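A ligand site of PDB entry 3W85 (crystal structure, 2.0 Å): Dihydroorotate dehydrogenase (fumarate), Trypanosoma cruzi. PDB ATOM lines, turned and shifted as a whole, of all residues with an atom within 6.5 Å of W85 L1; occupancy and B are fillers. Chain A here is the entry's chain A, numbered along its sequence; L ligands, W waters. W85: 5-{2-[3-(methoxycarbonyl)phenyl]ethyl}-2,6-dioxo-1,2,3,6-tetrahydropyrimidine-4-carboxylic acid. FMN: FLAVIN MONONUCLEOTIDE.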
ATOM      1  N   ALA A  20     -12.840  11.197 -32.053  1.00  0.00           N
ATOM      2  CA  ALA A  20     -12.020  10.020 -31.831  1.00  0.00           C
ATOM      3  C   ALA A  20     -11.457  10.009 -30.373  1.00  0.00           C
ATOM      4  O   ALA A  20     -11.077  11.055 -29.822  1.00  0.00           O
ATOM      5  CB  ALA A  20     -10.849  10.000 -32.798  1.00  0.00           C
ATOM      6  N   LYS A  44     -11.517   4.573 -31.943  1.00  0.00           N
ATOM      7  CA  LYS A  44     -10.278   5.063 -31.331  1.00  0.00           C
ATOM      8  C   LYS A  44      -9.053   5.007 -32.250  1.00  0.00           C
ATOM      9  O   LYS A  44      -8.778   3.971 -32.840  1.00  0.00           O
ATOM     10  CB  LYS A  44      -9.974   4.277 -30.050  1.00  0.00           C
ATOM     11  CG  LYS A  44      -8.613   4.514 -29.390  1.00  0.00           C
ATOM     12  CD  LYS A  44      -8.514   5.790 -28.568  1.00  0.00           C
ATOM     13  CE  LYS A  44      -7.049   6.186 -28.219  1.00  0.00           C
ATOM     14  NZ  LYS A  44      -6.999   7.566 -27.552  1.00  0.00           N
ATOM     15  N   SER A  45      -8.224   6.070 -32.200  1.00  0.00           N
ATOM     16  CA  SER A  45      -6.945   6.161 -32.968  1.00  0.00           C
ATOM     17  C   SER A  45      -6.082   4.962 -32.576  1.00  0.00           C
ATOM     18  O   SER A  45      -5.835   4.741 -31.410  1.00  0.00           O
ATOM     19  CB  SER A  45      -6.152   7.424 -32.674  1.00  0.00           C
ATOM     20  OG  SER A  45      -6.734   8.541 -33.268  1.00  0.00           O
ATOM     21  N   ARG A  51      -2.032  -1.163 -27.085  1.00  0.00           N
ATOM     22  CA  ARG A  51      -1.360  -0.369 -26.045  1.00  0.00           C
ATOM     23  C   ARG A  51      -2.204  -0.172 -24.818  1.00  0.00           C
ATOM     24  O   ARG A  51      -3.384   0.097 -24.923  1.00  0.00           O
ATOM     25  CB  ARG A  51      -1.019   1.049 -26.517  1.00  0.00           C
ATOM     26  CG  ARG A  51       0.058   1.091 -27.557  1.00  0.00           C
ATOM     27  CD  ARG A  51       0.142   2.461 -28.220  1.00  0.00           C
ATOM     28  NE  ARG A  51       0.416   3.491 -27.219  1.00  0.00           N
ATOM     29  CZ  ARG A  51       1.657   3.826 -26.835  1.00  0.00           C
ATOM     30  NH1 ARG A  51       2.688   3.178 -27.362  1.00  0.00           N
ATOM     31  NH2 ARG A  51       1.864   4.755 -25.919  1.00  0.00           N
ATOM     32  N   ASN A  54      -1.006   5.427 -20.832  1.00  0.00           N
ATOM     33  CA  ASN A  54      -0.353   6.011 -19.651  1.00  0.00           C
ATOM     34  C   ASN A  54      -0.991   5.553 -18.329  1.00  0.00           C
ATOM     35  O   ASN A  54      -2.185   5.126 -18.280  1.00  0.00           O
ATOM     36  CB  ASN A  54      -0.431   7.540 -19.755  1.00  0.00           C
ATOM     37  CG  ASN A  54       0.542   8.107 -20.744  1.00  0.00           C
ATOM     38  OD1 ASN A  54       1.482   7.431 -21.135  1.00  0.00           O
ATOM     39  ND2 ASN A  54       0.324   9.322 -21.157  1.00  0.00           N
ATOM     40  N   ASN A  68      -6.499  15.599 -20.663  1.00  0.00           N
ATOM     41  CA  ASN A  68      -6.153  14.178 -20.800  1.00  0.00           C
ATOM     42  C   ASN A  68      -4.702  13.987 -21.232  1.00  0.00           C
ATOM     43  O   ASN A  68      -4.195  14.733 -22.072  1.00  0.00           O
ATOM     44  CB  ASN A  68      -7.149  13.480 -21.776  1.00  0.00           C
ATOM     45  CG  ASN A  68      -6.703  13.520 -23.204  1.00  0.00           C
ATOM     46  OD1 ASN A  68      -5.788  12.769 -23.605  1.00  0.00           O
ATOM     47  ND2 ASN A  68      -7.360  14.376 -24.035  1.00  0.00           N
ATOM     48  N   SER A  69      -4.071  12.929 -20.733  1.00  0.00           N
ATOM     49  CA  SER A  69      -2.886  12.412 -21.335  1.00  0.00           C
ATOM     50  C   SER A  69      -2.993  10.908 -21.380  1.00  0.00           C
ATOM     51  O   SER A  69      -2.336  10.206 -20.604  1.00  0.00           O
ATOM     52  CB  SER A  69      -1.632  12.887 -20.577  1.00  0.00           C
ATOM     53  OG  SER A  69      -0.508  12.322 -21.244  1.00  0.00           O
ATOM     54  N   MET A  70      -3.870  10.406 -22.278  1.00  0.00           N
ATOM     55  CA  MET A  70      -4.217   8.972 -22.307  1.00  0.00           C
ATOM     56  C   MET A  70      -2.978   8.108 -22.735  1.00  0.00           C
ATOM     57  O   MET A  70      -2.789   6.981 -22.253  1.00  0.00           O
ATOM     58  CB  MET A  70      -5.376   8.737 -23.277  1.00  0.00           C
ATOM     59  CG  MET A  70      -6.652   9.537 -23.018  1.00  0.00           C
ATOM     60  SD  MET A  70      -7.375   9.282 -21.420  1.00  0.00           S
ATOM     61  CE  MET A  70      -8.019   7.615 -21.483  1.00  0.00           C
ATOM     62  N   GLY A  71      -2.130   8.618 -23.617  1.00  0.00           N
ATOM     63  CA  GLY A  71      -1.017   7.793 -24.162  1.00  0.00           C
ATOM     64  C   GLY A  71      -1.433   6.775 -25.229  1.00  0.00           C
ATOM     65  O   GLY A  71      -0.854   5.715 -25.338  1.00  0.00           O
ATOM     66  N   LEU A  72      -2.536   7.040 -25.929  1.00  0.00           N
ATOM     67  CA  LEU A  72      -2.990   6.192 -27.018  1.00  0.00           C
ATOM     68  C   LEU A  72      -3.230   4.725 -26.606  1.00  0.00           C
ATOM     69  O   LEU A  72      -2.830   3.809 -27.311  1.00  0.00           O
ATOM     70  CB  LEU A  72      -1.924   6.289 -28.133  1.00  0.00           C
ATOM     71  CG  LEU A  72      -2.283   6.224 -29.605  1.00  0.00           C
ATOM     72  CD1 LEU A  72      -3.644   6.847 -29.998  1.00  0.00           C
ATOM     73  CD2 LEU A  72      -1.076   6.832 -30.329  1.00  0.00           C
ATOM     74  N   PRO A  73      -3.957   4.508 -25.513  1.00  0.00           N
ATOM     75  CA  PRO A  73      -4.409   3.123 -25.207  1.00  0.00           C
ATOM     76  C   PRO A  73      -5.383   2.661 -26.285  1.00  0.00           C
ATOM     77  O   PRO A  73      -6.276   3.445 -26.689  1.00  0.00           O
ATOM     78  CB  PRO A  73      -5.181   3.300 -23.873  1.00  0.00           C
ATOM     79  CG  PRO A  73      -5.757   4.693 -23.943  1.00  0.00           C
ATOM     80  CD  PRO A  73      -4.662   5.526 -24.680  1.00  0.00           C
ATOM     81  N   SER A 100      -3.311   6.269 -35.887  1.00  0.00           N
ATOM     82  CA  SER A 100      -2.364   7.221 -35.350  1.00  0.00           C
ATOM     83  C   SER A 100      -1.023   6.528 -35.067  1.00  0.00           C
ATOM     84  O   SER A 100      -0.592   6.481 -33.884  1.00  0.00           O
ATOM     85  CB  SER A 100      -2.939   7.789 -34.060  1.00  0.00           C
ATOM     86  OG  SER A 100      -2.014   8.690 -33.532  1.00  0.00           O
ATOM     87  N   LEU A 102       2.971   5.520 -34.759  1.00  0.00           N
ATOM     88  CA  LEU A 102       4.065   6.266 -34.123  1.00  0.00           C
ATOM     89  C   LEU A 102       5.225   6.695 -35.054  1.00  0.00           C
ATOM     90  O   LEU A 102       6.156   7.331 -34.591  1.00  0.00           O
ATOM     91  CB  LEU A 102       4.616   5.516 -32.894  1.00  0.00           C
ATOM     92  CG  LEU A 102       3.602   5.145 -31.777  1.00  0.00           C
ATOM     93  CD1 LEU A 102       4.357   4.827 -30.496  1.00  0.00           C
ATOM     94  CD2 LEU A 102       2.594   6.269 -31.522  1.00  0.00           C
ATOM     95  N   ASN A 128      -4.664  10.670 -37.967  1.00  0.00           N
ATOM     96  CA  ASN A 128      -4.395  11.602 -36.909  1.00  0.00           C
ATOM     97  C   ASN A 128      -2.990  12.181 -37.006  1.00  0.00           C
ATOM     98  O   ASN A 128      -2.044  11.518 -36.734  1.00  0.00           O
ATOM     99  CB  ASN A 128      -4.625  10.919 -35.550  1.00  0.00           C
ATOM    100  CG  ASN A 128      -4.471  11.829 -34.356  1.00  0.00           C
ATOM    101  OD1 ASN A 128      -4.218  12.961 -34.461  1.00  0.00           O
ATOM    102  ND2 ASN A 128      -4.644  11.268 -33.211  1.00  0.00           N
ATOM    103  N   SER A 130      -2.054  14.914 -35.230  1.00  0.00           N
ATOM    104  CA  SER A 130      -1.843  15.630 -34.000  1.00  0.00           C
ATOM    105  C   SER A 130      -1.344  14.599 -33.095  1.00  0.00           C
ATOM    106  O   SER A 130      -2.031  14.166 -32.237  1.00  0.00           O
ATOM    107  CB  SER A 130      -3.133  16.279 -33.513  1.00  0.00           C
ATOM    108  OG  SER A 130      -4.195  16.164 -34.444  1.00  0.00           O
ATOM    109  N   CYS A 131      -0.139  14.124 -33.356  1.00  0.00           N
ATOM    110  CA  CYS A 131       0.402  12.920 -32.793  1.00  0.00           C
ATOM    111  C   CYS A 131       1.925  12.971 -32.652  1.00  0.00           C
ATOM    112  O   CYS A 131       2.598  13.564 -33.463  1.00  0.00           O
ATOM    113  CB  CYS A 131       0.029  11.777 -33.729  1.00  0.00           C
ATOM    114  SG  CYS A 131       1.080  10.320 -33.580  1.00  0.00           S
ATOM    115  N   PRO A 132       2.484  12.195 -31.603  1.00  0.00           N
ATOM    116  CA  PRO A 132       3.954  12.251 -31.507  1.00  0.00           C
ATOM    117  C   PRO A 132       4.744  11.663 -32.674  1.00  0.00           C
ATOM    118  O   PRO A 132       4.391  10.637 -33.187  1.00  0.00           O
ATOM    119  CB  PRO A 132       4.290  11.385 -30.274  1.00  0.00           C
ATOM    120  CG  PRO A 132       3.055  11.363 -29.467  1.00  0.00           C
ATOM    121  CD  PRO A 132       2.015  11.211 -30.502  1.00  0.00           C
ATOM    122  N   LYS A 165      -6.964  14.466 -39.137  1.00  0.00           N
ATOM    123  CA  LYS A 165      -7.311  15.213 -37.893  1.00  0.00           C
ATOM    124  C   LYS A 165      -6.159  16.135 -37.530  1.00  0.00           C
ATOM    125  O   LYS A 165      -5.017  15.707 -37.392  1.00  0.00           O
ATOM    126  CB  LYS A 165      -7.640  14.199 -36.797  1.00  0.00           C
ATOM    127  CG  LYS A 165      -7.834  14.761 -35.377  1.00  0.00           C
ATOM    128  CD  LYS A 165      -9.247  15.251 -35.174  1.00  0.00           C
ATOM    129  CE  LYS A 165      -9.534  15.457 -33.670  1.00  0.00           C
ATOM    130  NZ  LYS A 165      -9.881  14.203 -32.890  1.00  0.00           N
ATOM    131  N   ASN A 195      -8.007  18.799 -32.789  1.00  0.00           N
ATOM    132  CA  ASN A 195      -7.663  17.933 -31.724  1.00  0.00           C
ATOM    133  C   ASN A 195      -7.548  18.792 -30.474  1.00  0.00           C
ATOM    134  O   ASN A 195      -7.825  20.042 -30.497  1.00  0.00           O
ATOM    135  CB  ASN A 195      -6.350  17.165 -32.055  1.00  0.00           C
ATOM    136  CG  ASN A 195      -6.258  15.803 -31.349  1.00  0.00           C
ATOM    137  OD1 ASN A 195      -6.427  15.713 -30.150  1.00  0.00           O
ATOM    138  ND2 ASN A 195      -5.981  14.737 -32.127  1.00  0.00           N
ATOM    139  N   SER A 196      -7.189  18.163 -29.344  1.00  0.00           N
ATOM    140  CA  SER A 196      -7.089  18.906 -28.102  1.00  0.00           C
ATOM    141  C   SER A 196      -6.030  20.054 -28.116  1.00  0.00           C
ATOM    142  O   SER A 196      -5.059  20.054 -28.880  1.00  0.00           O
ATOM    143  CB  SER A 196      -6.929  17.908 -26.898  1.00  0.00           C
ATOM    144  OG  SER A 196      -5.743  17.164 -27.082  1.00  0.00           O
ATOM    145  N   LYS A 215       3.201  13.084 -17.316  1.00  0.00           N
ATOM    146  CA  LYS A 215       3.804  14.332 -17.847  1.00  0.00           C
ATOM    147  C   LYS A 215       3.664  15.471 -16.844  1.00  0.00           C
ATOM    148  O   LYS A 215       3.439  16.601 -17.220  1.00  0.00           O
ATOM    149  CB  LYS A 215       3.114  14.722 -19.200  1.00  0.00           C
ATOM    150  CG  LYS A 215       3.253  13.692 -20.342  1.00  0.00           C
ATOM    151  CD  LYS A 215       2.695  14.250 -21.666  1.00  0.00           C
ATOM    152  CE  LYS A 215       3.132  15.730 -21.863  1.00  0.00           C
ATOM    153  NZ  LYS A 215       2.638  16.332 -23.135  1.00  0.00           N
ATOM    154  N   GLY A 220      -3.761  17.446 -22.795  1.00  0.00           N
ATOM    155  CA  GLY A 220      -4.500  18.166 -23.817  1.00  0.00           C
ATOM    156  C   GLY A 220      -5.858  18.596 -23.297  1.00  0.00           C
ATOM    157  O   GLY A 220      -6.568  17.855 -22.595  1.00  0.00           O
ATOM    158  N   LEU A 221      -6.240  19.803 -23.681  1.00  0.00           N
ATOM    159  CA  LEU A 221      -7.465  20.423 -23.185  1.00  0.00           C
ATOM    160  C   LEU A 221      -8.634  20.260 -24.160  1.00  0.00           C
ATOM    161  O   LEU A 221      -8.457  20.457 -25.342  1.00  0.00           O
ATOM    162  CB  LEU A 221      -7.274  21.931 -23.002  1.00  0.00           C
ATOM    163  CG  LEU A 221      -6.163  22.405 -22.043  1.00  0.00           C
ATOM    164  CD1 LEU A 221      -5.943  23.953 -22.105  1.00  0.00           C
ATOM    165  CD2 LEU A 221      -6.342  21.875 -20.628  1.00  0.00           C
HETATM  166  OAB W85 L   1      -4.435   9.107 -26.501  1.00  0.00           O
HETATM  167  CAP W85 L   1      -4.218  10.344 -26.299  1.00  0.00           C
HETATM  168  OAF W85 L   1      -3.491  10.711 -25.340  1.00  0.00           O
HETATM  169  CAT W85 L   1      -4.738  11.403 -27.150  1.00  0.00           C
HETATM  170  NAM W85 L   1      -5.399  12.481 -26.490  1.00  0.00           N
HETATM  171  CAV W85 L   1      -5.889  13.613 -27.200  1.00  0.00           C
HETATM  172  OAD W85 L   1      -6.439  14.524 -26.571  1.00  0.00           O
HETATM  173  NAN W85 L   1      -5.730  13.629 -28.581  1.00  0.00           N
HETATM  174  CAW W85 L   1      -5.038  12.557 -29.267  1.00  0.00           C
HETATM  175  OAE W85 L   1      -4.913  12.611 -30.509  1.00  0.00           O
HETATM  176  CAU W85 L   1      -4.529  11.446 -28.515  1.00  0.00           C
HETATM  177  CAL W85 L   1      -3.844  10.379 -29.159  1.00  0.00           C
HETATM  178  CAK W85 L   1      -2.504  10.868 -29.888  1.00  0.00           C
HETATM  179  CAR W85 L   1      -1.536  11.179 -28.940  1.00  0.00           C
HETATM  180  CAJ W85 L   1      -0.667  10.181 -28.458  1.00  0.00           C
HETATM  181  CAH W85 L   1      -1.452  12.484 -28.393  1.00  0.00           C
HETATM  182  CAG W85 L   1      -0.490  12.800 -27.403  1.00  0.00           C
HETATM  183  CAI W85 L   1       0.387  11.806 -26.943  1.00  0.00           C
HETATM  184  CAS W85 L   1       0.304  10.482 -27.453  1.00  0.00           C
HETATM  185  CAQ W85 L   1       1.201   9.482 -26.963  1.00  0.00           C
HETATM  186  OAC W85 L   1       1.668   9.579 -25.817  1.00  0.00           O
HETATM  187  OAO W85 L   1       1.489   8.442 -27.817  1.00  0.00           O
HETATM  188  CAA W85 L   1       2.635   7.698 -27.350  1.00  0.00           C
HETATM  189  N1  FMN L   2      -8.215  12.675 -30.774  1.00  0.00           N
HETATM  190  C2  FMN L   2      -7.769  11.783 -31.716  1.00  0.00           C
HETATM  191  O2  FMN L   2      -7.604  12.161 -32.903  1.00  0.00           O
HETATM  192  N3  FMN L   2      -7.445  10.524 -31.410  1.00  0.00           N
HETATM  193  C4  FMN L   2      -7.611  10.029 -30.158  1.00  0.00           C
HETATM  194  O4  FMN L   2      -7.408   8.851 -29.808  1.00  0.00           O
HETATM  195  C4A FMN L   2      -8.143  10.882 -29.107  1.00  0.00           C
HETATM  196  N5  FMN L   2      -8.297  10.432 -27.860  1.00  0.00           N
HETATM  197  C5A FMN L   2      -8.915  11.212 -26.923  1.00  0.00           C
HETATM  198  C6  FMN L   2      -9.231  10.695 -25.657  1.00  0.00           C
HETATM  199  C7  FMN L   2      -9.850  11.516 -24.727  1.00  0.00           C
HETATM  200  C7M FMN L   2     -10.107  10.916 -23.366  1.00  0.00           C
HETATM  201  C8  FMN L   2     -10.213  12.923 -25.056  1.00  0.00           C
HETATM  202  C8M FMN L   2     -10.825  13.841 -24.022  1.00  0.00           C
HETATM  203  C9  FMN L   2      -9.921  13.415 -26.318  1.00  0.00           C
HETATM  204  C9A FMN L   2      -9.302  12.594 -27.248  1.00  0.00           C
HETATM  205  N10 FMN L   2      -8.995  13.095 -28.525  1.00  0.00           N
HETATM  206  C10 FMN L   2      -8.494  12.248 -29.517  1.00  0.00           C
HETATM  207  C1' FMN L   2      -9.344  14.464 -28.899  1.00  0.00           C
HETATM  208  C2' FMN L   2     -10.833  14.496 -29.177  1.00  0.00           C
HETATM  209  O2' FMN L   2     -10.999  13.808 -30.414  1.00  0.00           O
HETATM  210  C3' FMN L   2     -11.134  15.978 -29.511  1.00  0.00           C
HETATM  211  O3' FMN L   2     -10.387  16.346 -30.647  1.00  0.00           O
HETATM  212  C4' FMN L   2     -10.760  16.937 -28.409  1.00  0.00           C
HETATM  213  O4' FMN L   2     -11.191  16.358 -27.161  1.00  0.00           O
HETATM  214  C5' FMN L   2     -11.570  18.256 -28.634  1.00  0.00           C
HETATM  215  O5' FMN L   2     -13.030  18.136 -28.568  1.00  0.00           O
HETATM  216  P   FMN L   2     -14.045  18.433 -27.337  1.00  0.00           P
HETATM  217  O1P FMN L   2     -15.416  18.029 -27.779  1.00  0.00           O
HETATM  218  O2P FMN L   2     -13.690  19.850 -26.887  1.00  0.00           O
HETATM  219  O3P FMN L   2     -13.515  17.596 -26.181  1.00  0.00           O
HETATM  220  O   HOH W   1      -2.958  13.625 -24.758  1.00  0.00           O
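The backbone NH (N) of Met 70 is in hydrogen-bond range of the side-chain amide oxygen (OD1) of Asn 68 (3.3 Å). O of Met 70 sits at hydrogen-bond distance from N of Asn 54, at 2.8 Å. The side-chain hydroxyl (OG) of Ser 130 lies within hydrogen-bond range of the side-chain amide nitrogen (ND2) of Asn 195. The side-chain amide oxygen (OD1) of Asn 195 is in hydrogen-bond range of the side-chain hydroxyl (OG) of Ser 196, 3.5 Å away. The side-chain hydroxyl (OG) of Ser 130 sits at hydrogen-bond distance from the backbone carbonyl oxygen (O) of Lys 165. O of Asn 68 lies within hydrogen-bond range of N of Gly 220, 2.8 Å away. The backbone carbonyl oxygen (O) of Gly 71 lies within hydrogen-bond range of the guanidinium group (NH2) of Arg 51, at 2.9 Å. ND2 of Asn 128 is in hydrogen-bond range of OG of Ser 45, at 3.4 Å.
Water W1 bridges OAF of W85 L1 (3.0 Å) and O of Asn 68 (3.2 Å).
NH2 of Arg 51 touches CAA of W85 L1 (3.4 Å). Ser 69 touches W85 L1 (C to OAF, 3.996 Å). Ser 130 touches W85 L1 (O to OAE, 3.7 Å). Pro 132 touches W85 L1 (CG to CAS, 3.5 Å). Hydrophobic or aromatic side chains that line W85 L1: Met 70, Leu 72 and Pro 132. 12 residues have an atom within 4 Å of W85 L1: Lys 44, Arg 51, Asn 68, Ser 69, Met 70, Gly 71, Leu 72, Asn 128, Ser 130, Pro 132, Asn 195 and Ser 196. Along chain A the residues within 4 Å of W85 L1 span positions 44 to 196.
A nitrogen (N3) of FMN L2 sits close to an oxygen (OAE) of W85 L1.
The backbone carbonyl oxygen of Ala 20 lies within hydrogen-bond range of an oxygen (O2') of FMN L2 (2.8 Å). An oxygen (O2') of FMN L2 is in hydrogen-bond range of the side-chain amino group (NZ) of Lys 165 (2.7 Å). An oxygen (OAB) of W85 L1 is in salt-bridge range of the side-chain amino group (NZ) of Lys 44 (3.2 Å). ND2 of Asn 128 lies within hydrogen-bond range of O2 of FMN L2, 3.1 Å away. N of Met 70 sits at hydrogen-bond distance from OAF of W85 L1 (3.1 Å). The side-chain amide nitrogen (ND2) of Asn 128 is in hydrogen-bond range of an oxygen (OAE) of W85 L1, at 3.0 Å. O2 of FMN L2 is in hydrogen-bond range of ND2 of Asn 195 (3.1 Å). The side-chain amino group (NZ) of Lys 44 lies within hydrogen-bond range of an oxygen (O4) of FMN L2 (2.6 Å). OAB of W85 L1 sits at hydrogen-bond distance from N of Leu 72 (2.9 Å). N of Gly 71 sits at hydrogen-bond distance from OAF of W85 L1 (3.0 Å). The side-chain amide oxygen of Asn 195 lies within hydrogen-bond range of a nitrogen (NAN) of W85 L1, at 2.7 Å. An oxygen (OAD) of W85 L1 is in hydrogen-bond range of the side-chain amide nitrogen (ND2) of Asn 68, 2.7 Å away. N3 of FMN L2 sits at hydrogen-bond distance from OG of Ser 45 (2.8 Å). OAD of W85 L1 sits at hydrogen-bond distance from OG of Ser 196 (2.8 Å).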
